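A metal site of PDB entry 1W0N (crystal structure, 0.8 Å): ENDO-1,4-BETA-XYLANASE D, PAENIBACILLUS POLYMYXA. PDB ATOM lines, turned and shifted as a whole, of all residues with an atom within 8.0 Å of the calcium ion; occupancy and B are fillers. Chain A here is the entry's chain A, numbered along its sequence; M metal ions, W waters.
The calcium ion is bound by the side-chain carboxylate (OD1) of Asp 125 (2.3 Å), the side-chain carboxylate (OE1) of Glu 16 (2.3 Å), the backbone carbonyl oxygen (O) of Asp 35 (2.3 Å), water W1 (2.4 Å), the side-chain carboxylate (OE1) of Glu 18 (2.5 Å), the backbone carbonyl oxygen (O) of Asp 125 (2.5 Å) and the side-chain carboxylate (OE2) of Glu 18 (2.5 Å).
The backbone NH (N) of Ala 17 sits close to the backbone carbonyl oxygen (O) of Asp 125 (3.1 Å).
OD2 of Asp 125 is in salt-bridge range of NH1 of Arg 62.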
ATOM      1  N   LYS A  14      -5.089  30.940  -7.128  1.00  0.00           N
ATOM      2  CA  LYS A  14      -4.701  29.795  -7.941  1.00  0.00           C
ATOM      3  C   LYS A  14      -3.357  29.310  -7.470  1.00  0.00           C
ATOM      4  O   LYS A  14      -2.421  30.110  -7.323  1.00  0.00           O
ATOM      5  CB  LYS A  14      -4.649  30.207  -9.421  1.00  0.00           C
ATOM      6  CG  LYS A  14      -4.307  29.242 -10.384  1.00  0.00           C
ATOM      7  CD  LYS A  14      -4.452  29.794 -11.800  1.00  0.00           C
ATOM      8  CE  LYS A  14      -4.080  28.781 -12.829  1.00  0.00           C
ATOM      9  NZ  LYS A  14      -4.147  29.289 -14.201  1.00  0.00           N
ATOM     10  N   VAL A  15      -3.237  28.001  -7.236  1.00  0.00           N
ATOM     11  CA  VAL A  15      -1.976  27.384  -6.852  1.00  0.00           C
ATOM     12  C   VAL A  15      -1.712  26.236  -7.806  1.00  0.00           C
ATOM     13  O   VAL A  15      -2.556  25.354  -8.022  1.00  0.00           O
ATOM     14  CB  VAL A  15      -2.002  26.885  -5.395  1.00  0.00           C
ATOM     15  CG1 VAL A  15      -0.685  26.233  -5.026  1.00  0.00           C
ATOM     16  CG2 VAL A  15      -2.296  28.051  -4.448  1.00  0.00           C
ATOM     17  N   GLU A  16      -0.520  26.258  -8.425  1.00  0.00           N
ATOM     18  CA  GLU A  16      -0.122  25.212  -9.355  1.00  0.00           C
ATOM     19  C   GLU A  16       0.267  23.955  -8.599  1.00  0.00           C
ATOM     20  O   GLU A  16       1.005  24.011  -7.609  1.00  0.00           O
ATOM     21  CB  GLU A  16       1.065  25.696 -10.189  1.00  0.00           C
ATOM     22  CG  GLU A  16       0.773  26.896 -11.058  1.00  0.00           C
ATOM     23  CD  GLU A  16      -0.165  26.637 -12.223  1.00  0.00           C
ATOM     24  OE1 GLU A  16      -0.418  25.466 -12.532  1.00  0.00           O
ATOM     25  OE2 GLU A  16      -0.621  27.614 -12.834  1.00  0.00           O
ATOM     26  N   ALA A  17      -0.209  22.784  -9.059  1.00  0.00           N
ATOM     27  CA  ALA A  17       0.113  21.540  -8.378  1.00  0.00           C
ATOM     28  C   ALA A  17       1.621  21.311  -8.302  1.00  0.00           C
ATOM     29  O   ALA A  17       2.130  20.799  -7.300  1.00  0.00           O
ATOM     30  CB  ALA A  17      -0.569  20.378  -9.079  1.00  0.00           C
ATOM     31  N   GLU A  18       2.324  21.676  -9.378  1.00  0.00           N
ATOM     32  CA  GLU A  18       3.752  21.474  -9.476  1.00  0.00           C
ATOM     33  C   GLU A  18       4.538  22.343  -8.474  1.00  0.00           C
ATOM     34  O   GLU A  18       5.731  22.110  -8.319  1.00  0.00           O
ATOM     35  CB  GLU A  18       4.225  21.684 -10.912  1.00  0.00           C
ATOM     36  CG  GLU A  18       3.975  23.053 -11.526  1.00  0.00           C
ATOM     37  CD  GLU A  18       2.626  23.225 -12.251  1.00  0.00           C
ATOM     38  OE1 GLU A  18       1.622  22.587 -11.846  1.00  0.00           O
ATOM     39  OE2 GLU A  18       2.554  24.024 -13.209  1.00  0.00           O
ATOM     40  N   ASN A  19       3.881  23.288  -7.813  1.00  0.00           N
ATOM     41  CA  ASN A  19       4.504  24.090  -6.770  1.00  0.00           C
ATOM     42  C   ASN A  19       4.158  23.632  -5.353  1.00  0.00           C
ATOM     43  O   ASN A  19       4.600  24.237  -4.366  1.00  0.00           O
ATOM     44  CB  ASN A  19       4.144  25.563  -6.947  1.00  0.00           C
ATOM     45  CG  ASN A  19       4.718  26.142  -8.206  1.00  0.00           C
ATOM     46  OD1 ASN A  19       5.755  25.675  -8.698  1.00  0.00           O
ATOM     47  ND2 ASN A  19       4.090  27.176  -8.735  1.00  0.00           N
ATOM     48  N   ILE A  30       4.865  16.335 -13.717  1.00  0.00           N
ATOM     49  CA  ILE A  30       4.642  15.973 -15.107  1.00  0.00           C
ATOM     50  C   ILE A  30       4.671  17.220 -15.967  1.00  0.00           C
ATOM     51  O   ILE A  30       4.463  18.346 -15.482  1.00  0.00           O
ATOM     52  CB  ILE A  30       3.290  15.237 -15.295  1.00  0.00           C
ATOM     53  CG1 ILE A  30       2.104  16.122 -14.874  1.00  0.00           C
ATOM     54  CG2 ILE A  30       3.322  13.921 -14.534  1.00  0.00           C
ATOM     55  CD1 ILE A  30       0.732  15.500 -15.082  1.00  0.00           C
ATOM     56  N   PHE A  34      -0.130  18.523 -19.140  1.00  0.00           N
ATOM     57  CA  PHE A  34       0.114  19.899 -18.742  1.00  0.00           C
ATOM     58  C   PHE A  34       1.232  19.822 -17.715  1.00  0.00           C
ATOM     59  O   PHE A  34       1.598  18.745 -17.235  1.00  0.00           O
ATOM     60  CB  PHE A  34      -1.153  20.596 -18.174  1.00  0.00           C
ATOM     61  CG  PHE A  34      -2.001  19.681 -17.326  1.00  0.00           C
ATOM     62  CD1 PHE A  34      -1.486  19.113 -16.166  1.00  0.00           C
ATOM     63  CD2 PHE A  34      -3.289  19.378 -17.697  1.00  0.00           C
ATOM     64  CE1 PHE A  34      -2.257  18.244 -15.394  1.00  0.00           C
ATOM     65  CE2 PHE A  34      -4.083  18.527 -16.919  1.00  0.00           C
ATOM     66  CZ  PHE A  34      -3.547  17.950 -15.787  1.00  0.00           C
ATOM     67  N   ASP A  35       1.781  20.990 -17.354  1.00  0.00           N
ATOM     68  CA  ASP A  35       2.684  21.053 -16.212  1.00  0.00           C
ATOM     69  C   ASP A  35       1.858  20.877 -14.943  1.00  0.00           C
ATOM     70  O   ASP A  35       0.886  21.605 -14.709  1.00  0.00           O
ATOM     71  CB  ASP A  35       3.456  22.369 -16.215  1.00  0.00           C
ATOM     72  CG  ASP A  35       4.337  22.464 -17.453  1.00  0.00           C
ATOM     73  OD1 ASP A  35       5.182  21.572 -17.634  1.00  0.00           O
ATOM     74  OD2 ASP A  35       4.149  23.332 -18.304  1.00  0.00           O
ATOM     75  N   GLY A  36       2.209  19.878 -14.152  1.00  0.00           N
ATOM     76  CA  GLY A  36       1.393  19.527 -13.005  1.00  0.00           C
ATOM     77  C   GLY A  36       2.019  18.389 -12.265  1.00  0.00           C
ATOM     78  O   GLY A  36       3.250  18.225 -12.269  1.00  0.00           O
ATOM     79  N   VAL A  37       1.179  17.578 -11.599  1.00  0.00           N
ATOM     80  CA  VAL A  37       1.617  16.435 -10.843  1.00  0.00           C
ATOM     81  C   VAL A  37       0.692  15.259 -11.174  1.00  0.00           C
ATOM     82  O   VAL A  37      -0.523  15.460 -11.316  1.00  0.00           O
ATOM     83  CB  VAL A  37       1.649  16.711  -9.325  1.00  0.00           C
ATOM     84  CG1 VAL A  37       2.068  15.477  -8.528  1.00  0.00           C
ATOM     85  CG2 VAL A  37       2.570  17.876  -9.025  1.00  0.00           C
ATOM     86  N   ARG A  62      -8.199  21.885 -12.423  1.00  0.00           N
ATOM     87  CA  ARG A  62      -8.027  21.406 -13.784  1.00  0.00           C
ATOM     88  C   ARG A  62      -7.215  20.108 -13.719  1.00  0.00           C
ATOM     89  O   ARG A  62      -6.160  20.065 -13.086  1.00  0.00           O
ATOM     90  CB  ARG A  62      -7.331  22.446 -14.657  1.00  0.00           C
ATOM     91  CG  ARG A  62      -7.182  21.993 -16.094  1.00  0.00           C
ATOM     92  CD  ARG A  62      -6.760  23.124 -17.015  1.00  0.00           C
ATOM     93  NE  ARG A  62      -6.800  22.737 -18.418  1.00  0.00           N
ATOM     94  CZ  ARG A  62      -5.756  22.585 -19.232  1.00  0.00           C
ATOM     95  NH1 ARG A  62      -4.503  22.656 -18.790  1.00  0.00           N
ATOM     96  NH2 ARG A  62      -5.973  22.338 -20.534  1.00  0.00           N
ATOM     97  N   VAL A 124      -2.959  16.436 -12.342  1.00  0.00           N
ATOM     98  CA  VAL A 124      -3.500  17.616 -11.669  1.00  0.00           C
ATOM     99  C   VAL A 124      -2.699  18.812 -12.137  1.00  0.00           C
ATOM    100  O   VAL A 124      -1.448  18.793 -12.060  1.00  0.00           O
ATOM    101  CB  VAL A 124      -3.351  17.432 -10.127  1.00  0.00           C
ATOM    102  CG1 VAL A 124      -3.940  18.596  -9.420  1.00  0.00           C
ATOM    103  CG2 VAL A 124      -4.082  16.166  -9.660  1.00  0.00           C
ATOM    104  N   ASP A 125      -3.397  19.833 -12.627  1.00  0.00           N
ATOM    105  CA  ASP A 125      -2.718  21.021 -13.172  1.00  0.00           C
ATOM    106  C   ASP A 125      -2.600  22.121 -12.109  1.00  0.00           C
ATOM    107  O   ASP A 125      -1.498  22.609 -11.825  1.00  0.00           O
ATOM    108  CB  ASP A 125      -3.507  21.481 -14.400  1.00  0.00           C
ATOM    109  CG  ASP A 125      -2.889  22.643 -15.146  1.00  0.00           C
ATOM    110  OD1 ASP A 125      -1.831  23.140 -14.709  1.00  0.00           O
ATOM    111  OD2 ASP A 125      -3.470  23.076 -16.175  1.00  0.00           O
ATOM    112  N   PHE A 126      -3.735  22.497 -11.531  1.00  0.00           N
ATOM    113  CA  PHE A 126      -3.792  23.575 -10.540  1.00  0.00           C
ATOM    114  C   PHE A 126      -5.111  23.453  -9.787  1.00  0.00           C
ATOM    115  O   PHE A 126      -6.035  22.766 -10.230  1.00  0.00           O
ATOM    116  CB  PHE A 126      -3.674  24.965 -11.196  1.00  0.00           C
ATOM    117  CG  PHE A 126      -4.782  25.290 -12.167  1.00  0.00           C
ATOM    118  CD1 PHE A 126      -6.063  25.667 -11.727  1.00  0.00           C
ATOM    119  CD2 PHE A 126      -4.521  25.267 -13.537  1.00  0.00           C
ATOM    120  CE1 PHE A 126      -7.066  25.992 -12.634  1.00  0.00           C
ATOM    121  CE2 PHE A 126      -5.513  25.637 -14.450  1.00  0.00           C
ATOM    122  CZ  PHE A 126      -6.785  25.984 -13.983  1.00  0.00           C
ATOM    123  N   ILE A 127      -5.162  24.184  -8.667  1.00  0.00           N
ATOM    124  CA  ILE A 127      -6.381  24.388  -7.900  1.00  0.00           C
ATOM    125  C   ILE A 127      -6.660  25.886  -7.839  1.00  0.00           C
ATOM    126  O   ILE A 127      -5.736  26.696  -7.814  1.00  0.00           O
ATOM    127  CB  ILE A 127      -6.239  23.777  -6.467  1.00  0.00           C
ATOM    128  CG1 ILE A 127      -7.572  23.769  -5.721  1.00  0.00           C
ATOM    129  CG2 ILE A 127      -5.165  24.487  -5.662  1.00  0.00           C
ATOM    130  CD1 ILE A 127      -7.601  22.775  -4.572  1.00  0.00           C
HETATM  131 CA    CA M   1       0.109  23.486 -13.568  1.00  0.00          CA
HETATM  132  O   HOH W   1       0.531  24.819 -15.547  1.00  0.00           O
